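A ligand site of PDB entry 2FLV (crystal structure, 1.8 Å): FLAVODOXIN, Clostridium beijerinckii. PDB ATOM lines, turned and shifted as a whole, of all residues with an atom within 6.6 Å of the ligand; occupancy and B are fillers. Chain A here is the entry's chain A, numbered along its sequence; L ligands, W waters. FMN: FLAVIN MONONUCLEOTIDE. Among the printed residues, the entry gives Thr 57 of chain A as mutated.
The side-chain carboxylate (OE1) of Glu 59 is in hydrogen-bond range of the backbone NH (N) of Trp 95 (3.0 Å). The backbone NH (N) of Gly 10 sits at hydrogen-bond distance from the side-chain hydroxyl (OG) of Ser 7 (2.9 Å). The backbone NH (N) of Ser 87 sits at hydrogen-bond distance from the side-chain hydroxyl (OG1) of Thr 12. OG of Ser 87 sits at hydrogen-bond distance from O of Asn 119 (2.7 Å). The side-chain amide nitrogen (NE2) of Gln 118 lies within hydrogen-bond range of the backbone carbonyl oxygen (O) of Gly 89 (3.1 Å). O of Tyr 88 is in hydrogen-bond range of N of Asn 119, at 2.9 Å. N of Tyr 88 sits at hydrogen-bond distance from O of Val 117, at 3.1 Å. The side-chain amide nitrogen (ND2) of Asn 119 lies close to the side-chain amide nitrogen (NE2) of Gln 118 (3.5 Å).
Merely in contact with the ligand: Met 56 (3.4 Å), Asp 58 (3.4 Å), Tyr 88 (3.5 Å), Asn 119 (3.5 Å) and Trp 6 (3.9 Å). Hydrophobic or aromatic side chains within 4 Å of the ligand: Trp 6, Ala 55, Met 56, Tyr 88 and Trp 90. Of the 29 residues printed, 19 come within 4 Å of the ligand.
An oxygen (O1P) of the ligand lies within hydrogen-bond range of the backbone NH of Thr 9. OG1 of Thr 9 is in hydrogen-bond range of O1P of the ligand (2.6 Å). N of Glu 59 is in hydrogen-bond range of O4 of the ligand (2.7 Å). OE2 of Glu 59 sits at hydrogen-bond distance from N3 of the ligand. The side-chain hydroxyl (OG) of Ser 7 lies within hydrogen-bond range of an oxygen (O2P) of the ligand, 2.7 Å away. N of Gly 91 is in hydrogen-bond range of O2 of the ligand. OG of Ser 87 lies within hydrogen-bond range of O4' of the ligand, 2.7 Å away. The backbone NH of Asn 11 sits at hydrogen-bond distance from an oxygen (O1P) of the ligand, at 2.9 Å. The side-chain amide oxygen (OD1) of Asn 11 is in hydrogen-bond range of an oxygen (O4') of the ligand (2.7 Å). N of Gly 8 sits at hydrogen-bond distance from O3P of the ligand, 2.7 Å away. The backbone NH (N) of Thr 12 sits at hydrogen-bond distance from an oxygen (O2P) of the ligand (2.8 Å). The side-chain hydroxyl (OG1) of Thr 12 is in hydrogen-bond range of an oxygen (O2P) of the ligand, at 2.8 Å. The backbone NH (N) of Thr 57 lies close to a nitrogen (N5) of the ligand (3.4 Å). The side-chain hydroxyl (OG) of Ser 54 lies within hydrogen-bond range of an oxygen (O3P) of the ligand (2.8 Å). N of Ala 55 is in hydrogen-bond range of O2' of the ligand, 3.4 Å away. The backbone carbonyl oxygen (O) of Ala 55 is in hydrogen-bond range of an oxygen (O2') of the ligand, 2.8 Å away. The backbone NH (N) of Trp 90 lies within hydrogen-bond range of an oxygen (O2) of the ligand, at 3.0 Å. N1 of the ligand lies within hydrogen-bond range of N of Gly 89 (3.0 Å). The backbone NH of Gly 10 sits at hydrogen-bond distance from an oxygen (O1P) of the ligand (3.0 Å).
Water W2 lies within hydrogen-bond range of an oxygen (O3') of the ligand, the side-chain amide oxygen (OD1) of Asn 119 and the side-chain amide oxygen (OD1) of Asn 11. Water W3 lies within hydrogen-bond range of O4 of the ligand (2.7 Å), NE1 of Trp 90 (2.9 Å) and OD1 of Asp 58 (3.1 Å). Water W4 lies within hydrogen-bond range of N of Gly 93, OE1 of Glu 59, O2 of the ligand and N of Asp 92.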
ATOM      1  N   TRP A   6      25.207 -33.525 -29.538  1.00  0.00           N
ATOM      2  CA  TRP A   6      25.838 -34.079 -28.334  1.00  0.00           C
ATOM      3  C   TRP A   6      24.959 -33.536 -27.191  1.00  0.00           C
ATOM      4  O   TRP A   6      24.585 -32.357 -27.197  1.00  0.00           O
ATOM      5  CB  TRP A   6      27.280 -33.603 -28.130  1.00  0.00           C
ATOM      6  CG  TRP A   6      27.910 -34.251 -26.908  1.00  0.00           C
ATOM      7  CD1 TRP A   6      28.571 -35.456 -26.877  1.00  0.00           C
ATOM      8  CD2 TRP A   6      27.820 -33.818 -25.540  1.00  0.00           C
ATOM      9  NE1 TRP A   6      28.877 -35.796 -25.576  1.00  0.00           N
ATOM     10  CE2 TRP A   6      28.429 -34.813 -24.734  1.00  0.00           C
ATOM     11  CE3 TRP A   6      27.284 -32.679 -24.906  1.00  0.00           C
ATOM     12  CZ2 TRP A   6      28.503 -34.717 -23.338  1.00  0.00           C
ATOM     13  CZ3 TRP A   6      27.359 -32.582 -23.510  1.00  0.00           C
ATOM     14  CH2 TRP A   6      27.961 -33.596 -22.741  1.00  0.00           C
ATOM     15  N   SER A   7      24.609 -34.401 -26.246  1.00  0.00           N
ATOM     16  CA  SER A   7      23.794 -34.004 -25.097  1.00  0.00           C
ATOM     17  C   SER A   7      24.290 -34.708 -23.832  1.00  0.00           C
ATOM     18  O   SER A   7      24.478 -35.925 -23.830  1.00  0.00           O
ATOM     19  CB  SER A   7      22.315 -34.334 -25.362  1.00  0.00           C
ATOM     20  OG  SER A   7      21.468 -33.829 -24.344  1.00  0.00           O
ATOM     21  N   GLY A   8      24.487 -33.959 -22.765  1.00  0.00           N
ATOM     22  CA  GLY A   8      24.968 -34.550 -21.529  1.00  0.00           C
ATOM     23  C   GLY A   8      23.898 -35.023 -20.582  1.00  0.00           C
ATOM     24  O   GLY A   8      24.115 -35.950 -19.822  1.00  0.00           O
ATOM     25  N   THR A   9      22.730 -34.379 -20.606  1.00  0.00           N
ATOM     26  CA  THR A   9      21.636 -34.779 -19.725  1.00  0.00           C
ATOM     27  C   THR A   9      20.317 -34.993 -20.488  1.00  0.00           C
ATOM     28  O   THR A   9      19.288 -35.359 -19.907  1.00  0.00           O
ATOM     29  CB  THR A   9      21.397 -33.743 -18.587  1.00  0.00           C
ATOM     30  OG1 THR A   9      20.715 -32.591 -19.107  1.00  0.00           O
ATOM     31  CG2 THR A   9      22.715 -33.308 -17.946  1.00  0.00           C
ATOM     32  N   GLY A  10      20.340 -34.724 -21.793  1.00  0.00           N
ATOM     33  CA  GLY A  10      19.151 -34.917 -22.604  1.00  0.00           C
ATOM     34  C   GLY A  10      18.473 -33.637 -23.056  1.00  0.00           C
ATOM     35  O   GLY A  10      17.527 -33.712 -23.845  1.00  0.00           O
ATOM     36  N   ASN A  11      18.966 -32.473 -22.655  1.00  0.00           N
ATOM     37  CA  ASN A  11      18.298 -31.243 -23.067  1.00  0.00           C
ATOM     38  C   ASN A  11      18.438 -30.956 -24.556  1.00  0.00           C
ATOM     39  O   ASN A  11      17.421 -30.696 -25.238  1.00  0.00           O
ATOM     40  CB  ASN A  11      18.754 -30.052 -22.225  1.00  0.00           C
ATOM     41  CG  ASN A  11      18.341 -30.166 -20.762  1.00  0.00           C
ATOM     42  OD1 ASN A  11      18.954 -29.557 -19.882  1.00  0.00           O
ATOM     43  ND2 ASN A  11      17.319 -30.956 -20.495  1.00  0.00           N
ATOM     44  N   THR A  12      19.666 -31.037 -25.069  1.00  0.00           N
ATOM     45  CA  THR A  12      19.922 -30.815 -26.490  1.00  0.00           C
ATOM     46  C   THR A  12      19.305 -31.965 -27.310  1.00  0.00           C
ATOM     47  O   THR A  12      18.849 -31.751 -28.426  1.00  0.00           O
ATOM     48  CB  THR A  12      21.437 -30.663 -26.777  1.00  0.00           C
ATOM     49  OG1 THR A  12      21.938 -29.552 -26.024  1.00  0.00           O
ATOM     50  CG2 THR A  12      21.685 -30.383 -28.242  1.00  0.00           C
ATOM     51  N   GLU A  13      19.275 -33.155 -26.733  1.00  0.00           N
ATOM     52  CA  GLU A  13      18.686 -34.317 -27.395  1.00  0.00           C
ATOM     53  C   GLU A  13      17.182 -34.063 -27.631  1.00  0.00           C
ATOM     54  O   GLU A  13      16.651 -34.335 -28.713  1.00  0.00           O
ATOM     55  CB  GLU A  13      18.867 -35.572 -26.549  1.00  0.00           C
ATOM     56  CG  GLU A  13      18.338 -36.835 -27.208  1.00  0.00           C
ATOM     57  CD  GLU A  13      18.519 -38.089 -26.361  1.00  0.00           C
ATOM     58  OE1 GLU A  13      18.750 -37.974 -25.135  1.00  0.00           O
ATOM     59  OE2 GLU A  13      18.409 -39.187 -26.918  1.00  0.00           O
ATOM     60  N   CYS A  53      24.763 -28.794 -29.742  1.00  0.00           N
ATOM     61  CA  CYS A  53      25.617 -29.131 -28.595  1.00  0.00           C
ATOM     62  C   CYS A  53      25.395 -28.107 -27.518  1.00  0.00           C
ATOM     63  O   CYS A  53      25.343 -26.908 -27.786  1.00  0.00           O
ATOM     64  CB  CYS A  53      27.100 -29.132 -28.983  1.00  0.00           C
ATOM     65  SG  CYS A  53      28.259 -29.599 -27.637  1.00  0.00           S
ATOM     66  N   SER A  54      25.252 -28.572 -26.297  1.00  0.00           N
ATOM     67  CA  SER A  54      25.045 -27.710 -25.153  1.00  0.00           C
ATOM     68  C   SER A  54      26.321 -26.950 -24.776  1.00  0.00           C
ATOM     69  O   SER A  54      27.422 -27.285 -25.226  1.00  0.00           O
ATOM     70  CB  SER A  54      24.583 -28.547 -23.957  1.00  0.00           C
ATOM     71  OG  SER A  54      25.483 -29.622 -23.715  1.00  0.00           O
ATOM     72  N   ALA A  55      26.162 -25.918 -23.939  1.00  0.00           N
ATOM     73  CA  ALA A  55      27.299 -25.127 -23.487  1.00  0.00           C
ATOM     74  C   ALA A  55      28.069 -25.953 -22.464  1.00  0.00           C
ATOM     75  O   ALA A  55      27.479 -26.523 -21.541  1.00  0.00           O
ATOM     76  CB  ALA A  55      26.812 -23.832 -22.867  1.00  0.00           C
ATOM     77  N   MET A  56      29.381 -26.051 -22.640  1.00  0.00           N
ATOM     78  CA  MET A  56      30.221 -26.834 -21.728  1.00  0.00           C
ATOM     79  C   MET A  56      31.320 -26.019 -21.052  1.00  0.00           C
ATOM     80  O   MET A  56      31.729 -24.962 -21.537  1.00  0.00           O
ATOM     81  CB  MET A  56      30.841 -28.044 -22.442  1.00  0.00           C
ATOM     82  CG  MET A  56      30.173 -29.380 -22.132  1.00  0.00           C
ATOM     83  SD  MET A  56      30.340 -29.894 -20.390  1.00  0.00           S
ATOM     84  CE  MET A  56      32.073 -29.645 -20.107  1.00  0.00           C
ATOM     85  N   THR A  57      31.771 -26.542 -19.913  1.00  0.00           N
ATOM     86  CA  THR A  57      32.805 -25.936 -19.069  1.00  0.00           C
ATOM     87  C   THR A  57      32.545 -24.445 -18.929  1.00  0.00           C
ATOM     88  O   THR A  57      31.672 -24.040 -18.167  1.00  0.00           O
ATOM     89  CB  THR A  57      34.225 -26.250 -19.609  1.00  0.00           C
ATOM     90  OG1 THR A  57      34.294 -27.611 -20.041  1.00  0.00           O
ATOM     91  CG2 THR A  57      35.255 -26.031 -18.504  1.00  0.00           C
ATOM     92  N   ASP A  58      33.233 -23.634 -19.715  1.00  0.00           N
ATOM     93  CA  ASP A  58      33.012 -22.192 -19.672  1.00  0.00           C
ATOM     94  C   ASP A  58      32.768 -21.667 -21.059  1.00  0.00           C
ATOM     95  O   ASP A  58      33.700 -21.235 -21.764  1.00  0.00           O
ATOM     96  CB  ASP A  58      34.174 -21.460 -19.001  1.00  0.00           C
ATOM     97  CG  ASP A  58      34.203 -21.665 -17.499  1.00  0.00           C
ATOM     98  OD1 ASP A  58      33.131 -21.580 -16.862  1.00  0.00           O
ATOM     99  OD2 ASP A  58      35.298 -21.929 -16.946  1.00  0.00           O
ATOM    100  N   GLU A  59      31.526 -21.789 -21.501  1.00  0.00           N
ATOM    101  CA  GLU A  59      31.093 -21.309 -22.798  1.00  0.00           C
ATOM    102  C   GLU A  59      31.848 -21.868 -24.010  1.00  0.00           C
ATOM    103  O   GLU A  59      32.260 -21.106 -24.893  1.00  0.00           O
ATOM    104  CB  GLU A  59      31.115 -19.777 -22.831  1.00  0.00           C
ATOM    105  CG  GLU A  59      30.270 -19.096 -21.762  1.00  0.00           C
ATOM    106  CD  GLU A  59      28.769 -19.299 -21.927  1.00  0.00           C
ATOM    107  OE1 GLU A  59      28.300 -19.543 -23.065  1.00  0.00           O
ATOM    108  OE2 GLU A  59      28.047 -19.177 -20.916  1.00  0.00           O
ATOM    109  N   VAL A  60      32.043 -23.182 -24.058  1.00  0.00           N
ATOM    110  CA  VAL A  60      32.711 -23.801 -25.198  1.00  0.00           C
ATOM    111  C   VAL A  60      31.920 -25.029 -25.622  1.00  0.00           C
ATOM    112  O   VAL A  60      30.957 -25.413 -24.945  1.00  0.00           O
ATOM    113  CB  VAL A  60      34.179 -24.221 -24.897  1.00  0.00           C
ATOM    114  CG1 VAL A  60      35.003 -23.007 -24.508  1.00  0.00           C
ATOM    115  CG2 VAL A  60      34.222 -25.304 -23.800  1.00  0.00           C
ATOM    116  N   GLY A  86      21.351 -25.629 -29.539  1.00  0.00           N
ATOM    117  CA  GLY A  86      21.856 -26.191 -28.306  1.00  0.00           C
ATOM    118  C   GLY A  86      21.213 -25.594 -27.071  1.00  0.00           C
ATOM    119  O   GLY A  86      20.663 -24.492 -27.106  1.00  0.00           O
ATOM    120  N   SER A  87      21.292 -26.339 -25.976  1.00  0.00           N
ATOM    121  CA  SER A  87      20.743 -25.940 -24.693  1.00  0.00           C
ATOM    122  C   SER A  87      21.894 -25.372 -23.840  1.00  0.00           C
ATOM    123  O   SER A  87      23.062 -25.755 -23.995  1.00  0.00           O
ATOM    124  CB  SER A  87      20.118 -27.161 -24.007  1.00  0.00           C
ATOM    125  OG  SER A  87      19.481 -26.817 -22.792  1.00  0.00           O
ATOM    126  N   TYR A  88      21.564 -24.445 -22.936  1.00  0.00           N
ATOM    127  CA  TYR A  88      22.545 -23.828 -22.067  1.00  0.00           C
ATOM    128  C   TYR A  88      21.913 -23.628 -20.692  1.00  0.00           C
ATOM    129  O   TYR A  88      20.683 -23.761 -20.553  1.00  0.00           O
ATOM    130  CB  TYR A  88      23.046 -22.509 -22.656  1.00  0.00           C
ATOM    131  CG  TYR A  88      21.993 -21.440 -22.746  1.00  0.00           C
ATOM    132  CD1 TYR A  88      21.032 -21.456 -23.752  1.00  0.00           C
ATOM    133  CD2 TYR A  88      21.966 -20.396 -21.825  1.00  0.00           C
ATOM    134  CE1 TYR A  88      20.072 -20.464 -23.849  1.00  0.00           C
ATOM    135  CE2 TYR A  88      21.006 -19.395 -21.905  1.00  0.00           C
ATOM    136  CZ  TYR A  88      20.074 -19.433 -22.919  1.00  0.00           C
ATOM    137  OH  TYR A  88      19.143 -18.434 -22.995  1.00  0.00           O
ATOM    138  N   GLY A  89      22.728 -23.286 -19.706  1.00  0.00           N
ATOM    139  CA  GLY A  89      22.194 -23.157 -18.364  1.00  0.00           C
ATOM    140  C   GLY A  89      22.191 -21.838 -17.628  1.00  0.00           C
ATOM    141  O   GLY A  89      21.162 -21.449 -17.076  1.00  0.00           O
ATOM    142  N   TRP A  90      23.334 -21.181 -17.548  1.00  0.00           N
ATOM    143  CA  TRP A  90      23.417 -19.917 -16.821  1.00  0.00           C
ATOM    144  C   TRP A  90      23.932 -18.732 -17.610  1.00  0.00           C
ATOM    145  O   TRP A  90      23.884 -17.592 -17.134  1.00  0.00           O
ATOM    146  CB  TRP A  90      24.261 -20.091 -15.547  1.00  0.00           C
ATOM    147  CG  TRP A  90      25.591 -20.720 -15.806  1.00  0.00           C
ATOM    148  CD1 TRP A  90      26.712 -20.117 -16.282  1.00  0.00           C
ATOM    149  CD2 TRP A  90      25.938 -22.106 -15.618  1.00  0.00           C
ATOM    150  NE1 TRP A  90      27.740 -21.019 -16.401  1.00  0.00           N
ATOM    151  CE2 TRP A  90      27.293 -22.250 -15.994  1.00  0.00           C
ATOM    152  CE3 TRP A  90      25.243 -23.237 -15.171  1.00  0.00           C
ATOM    153  CZ2 TRP A  90      27.959 -23.477 -15.938  1.00  0.00           C
ATOM    154  CZ3 TRP A  90      25.900 -24.450 -15.113  1.00  0.00           C
ATOM    155  CH2 TRP A  90      27.249 -24.562 -15.496  1.00  0.00           C
ATOM    156  N   GLY A  91      24.451 -18.994 -18.799  1.00  0.00           N
ATOM    157  CA  GLY A  91      24.978 -17.919 -19.617  1.00  0.00           C
ATOM    158  C   GLY A  91      23.889 -17.314 -20.473  1.00  0.00           C
ATOM    159  O   GLY A  91      22.699 -17.475 -20.202  1.00  0.00           O
ATOM    160  N   ASP A  92      24.297 -16.589 -21.508  1.00  0.00           N
ATOM    161  CA  ASP A  92      23.339 -15.968 -22.419  1.00  0.00           C
ATOM    162  C   ASP A  92      23.637 -16.287 -23.892  1.00  0.00           C
ATOM    163  O   ASP A  92      23.290 -15.521 -24.779  1.00  0.00           O
ATOM    164  CB  ASP A  92      23.230 -14.464 -22.184  1.00  0.00           C
ATOM    165  CG  ASP A  92      24.557 -13.730 -22.350  1.00  0.00           C
ATOM    166  OD1 ASP A  92      25.497 -14.283 -22.978  1.00  0.00           O
ATOM    167  OD2 ASP A  92      24.658 -12.592 -21.849  1.00  0.00           O
ATOM    168  N   GLY A  93      24.345 -17.388 -24.121  1.00  0.00           N
ATOM    169  CA  GLY A  93      24.640 -17.798 -25.486  1.00  0.00           C
ATOM    170  C   GLY A  93      26.034 -17.573 -26.018  1.00  0.00           C
ATOM    171  O   GLY A  93      26.231 -17.744 -27.226  1.00  0.00           O
ATOM    172  N   TRP A  95      28.770 -19.425 -25.993  1.00  0.00           N
ATOM    173  CA  TRP A  95      29.315 -20.577 -26.710  1.00  0.00           C
ATOM    174  C   TRP A  95      28.735 -20.669 -28.114  1.00  0.00           C
ATOM    175  O   TRP A  95      29.436 -21.016 -29.059  1.00  0.00           O
ATOM    176  CB  TRP A  95      29.101 -21.894 -25.917  1.00  0.00           C
ATOM    177  CG  TRP A  95      27.956 -22.760 -26.363  1.00  0.00           C
ATOM    178  CD1 TRP A  95      28.037 -23.967 -26.994  1.00  0.00           C
ATOM    179  CD2 TRP A  95      26.549 -22.494 -26.184  1.00  0.00           C
ATOM    180  NE1 TRP A  95      26.787 -24.473 -27.212  1.00  0.00           N
ATOM    181  CE2 TRP A  95      25.851 -23.592 -26.742  1.00  0.00           C
ATOM    182  CE3 TRP A  95      25.821 -21.440 -25.622  1.00  0.00           C
ATOM    183  CZ2 TRP A  95      24.453 -23.666 -26.741  1.00  0.00           C
ATOM    184  CZ3 TRP A  95      24.424 -21.514 -25.621  1.00  0.00           C
ATOM    185  CH2 TRP A  95      23.755 -22.615 -26.175  1.00  0.00           C
ATOM    186  N   VAL A 117      18.165 -22.687 -26.226  1.00  0.00           N
ATOM    187  CA  VAL A 117      17.085 -22.834 -25.255  1.00  0.00           C
ATOM    188  C   VAL A 117      17.713 -23.122 -23.900  1.00  0.00           C
ATOM    189  O   VAL A 117      18.654 -23.910 -23.815  1.00  0.00           O
ATOM    190  CB  VAL A 117      16.156 -24.006 -25.663  1.00  0.00           C
ATOM    191  CG1 VAL A 117      15.162 -24.329 -24.565  1.00  0.00           C
ATOM    192  CG2 VAL A 117      15.414 -23.649 -26.950  1.00  0.00           C
ATOM    193  N   GLN A 118      17.189 -22.494 -22.845  1.00  0.00           N
ATOM    194  CA  GLN A 118      17.728 -22.696 -21.511  1.00  0.00           C
ATOM    195  C   GLN A 118      17.165 -23.953 -20.870  1.00  0.00           C
ATOM    196  O   GLN A 118      15.938 -24.100 -20.758  1.00  0.00           O
ATOM    197  CB  GLN A 118      17.470 -21.481 -20.623  1.00  0.00           C
ATOM    198  CG  GLN A 118      18.239 -21.520 -19.293  1.00  0.00           C
ATOM    199  CD  GLN A 118      18.014 -20.303 -18.415  1.00  0.00           C
ATOM    200  OE1 GLN A 118      17.644 -19.225 -18.903  1.00  0.00           O
ATOM    201  NE2 GLN A 118      18.246 -20.451 -17.100  1.00  0.00           N
ATOM    202  N   ASN A 119      18.051 -24.855 -20.461  1.00  0.00           N
ATOM    203  CA  ASN A 119      17.669 -26.118 -19.814  1.00  0.00           C
ATOM    204  C   ASN A 119      16.775 -26.958 -20.747  1.00  0.00           C
ATOM    205  O   ASN A 119      16.937 -26.900 -21.970  1.00  0.00           O
ATOM    206  CB  ASN A 119      16.988 -25.846 -18.471  1.00  0.00           C
ATOM    207  CG  ASN A 119      17.783 -24.871 -17.597  1.00  0.00           C
ATOM    208  OD1 ASN A 119      18.933 -25.128 -17.228  1.00  0.00           O
ATOM    209  ND2 ASN A 119      17.172 -23.729 -17.303  1.00  0.00           N
ATOM    210  N   GLU A 120      15.857 -27.752 -20.196  1.00  0.00           N
ATOM    211  CA  GLU A 120      14.976 -28.550 -21.048  1.00  0.00           C
ATOM    212  C   GLU A 120      14.003 -27.588 -21.737  1.00  0.00           C
ATOM    213  O   GLU A 120      13.483 -26.676 -21.092  1.00  0.00           O
ATOM    214  CB  GLU A 120      14.219 -29.614 -20.242  1.00  0.00           C
ATOM    215  CG  GLU A 120      13.578 -30.692 -21.127  1.00  0.00           C
ATOM    216  CD  GLU A 120      12.786 -31.749 -20.363  1.00  0.00           C
ATOM    217  OE1 GLU A 120      13.370 -32.403 -19.485  1.00  0.00           O
ATOM    218  OE2 GLU A 120      11.580 -31.930 -20.666  1.00  0.00           O
HETATM  219  N1  FMN L   1      25.702 -23.450 -19.395  1.00  0.00           N
HETATM  220  C2  FMN L   1      25.978 -22.177 -19.781  1.00  0.00           C
HETATM  221  O2  FMN L   1      25.081 -21.384 -19.970  1.00  0.00           O
HETATM  222  N3  FMN L   1      27.317 -21.819 -19.956  1.00  0.00           N
HETATM  223  C4  FMN L   1      28.420 -22.599 -19.632  1.00  0.00           C
HETATM  224  O4  FMN L   1      29.578 -22.191 -19.711  1.00  0.00           O
HETATM  225  C4A FMN L   1      28.105 -23.973 -19.193  1.00  0.00           C
HETATM  226  N5  FMN L   1      29.084 -24.811 -18.824  1.00  0.00           N
HETATM  227  C5A FMN L   1      28.698 -26.016 -18.244  1.00  0.00           C
HETATM  228  C6  FMN L   1      29.669 -26.897 -17.703  1.00  0.00           C
HETATM  229  C7  FMN L   1      29.338 -28.144 -17.267  1.00  0.00           C
HETATM  230  C7M FMN L   1      30.386 -29.097 -16.749  1.00  0.00           C
HETATM  231  C8  FMN L   1      27.978 -28.569 -17.286  1.00  0.00           C
HETATM  232  C8M FMN L   1      27.581 -29.972 -16.861  1.00  0.00           C
HETATM  233  C9  FMN L   1      26.981 -27.714 -17.734  1.00  0.00           C
HETATM  234  C9A FMN L   1      27.321 -26.457 -18.233  1.00  0.00           C
HETATM  235  N10 FMN L   1      26.343 -25.553 -18.627  1.00  0.00           N
HETATM  236  C10 FMN L   1      26.670 -24.306 -19.109  1.00  0.00           C
HETATM  237  C1' FMN L   1      24.934 -25.941 -18.487  1.00  0.00           C
HETATM  238  C2' FMN L   1      24.417 -26.833 -19.626  1.00  0.00           C
HETATM  239  O2' FMN L   1      24.732 -26.215 -20.872  1.00  0.00           O
HETATM  240  C3' FMN L   1      22.887 -26.961 -19.514  1.00  0.00           C
HETATM  241  O3' FMN L   1      22.551 -27.635 -18.295  1.00  0.00           O
HETATM  242  C4' FMN L   1      22.176 -27.635 -20.697  1.00  0.00           C
HETATM  243  O4' FMN L   1      20.764 -27.584 -20.491  1.00  0.00           O
HETATM  244  C5' FMN L   1      22.641 -29.089 -20.829  1.00  0.00           C
HETATM  245  O5' FMN L   1      22.190 -29.639 -22.037  1.00  0.00           O
HETATM  246  P   FMN L   1      22.421 -31.154 -22.360  1.00  0.00           P
HETATM  247  O1P FMN L   1      21.632 -32.037 -21.485  1.00  0.00           O
HETATM  248  O2P FMN L   1      22.118 -31.236 -23.782  1.00  0.00           O
HETATM  249  O3P FMN L   1      23.928 -31.338 -22.164  1.00  0.00           O
HETATM  250  O   HOH W   1      25.468 -31.315 -19.891  1.00  0.00           O
HETATM  251  O   HOH W   2      20.120 -27.611 -17.409  1.00  0.00           O
HETATM  252  O   HOH W   3      30.320 -20.550 -17.709  1.00  0.00           O
HETATM  253  O   HOH W   4      25.395 -19.682 -22.699  1.00  0.00           O
HETATM  254  O   HOH W   5      24.110 -30.011 -17.923  1.00  0.00           O
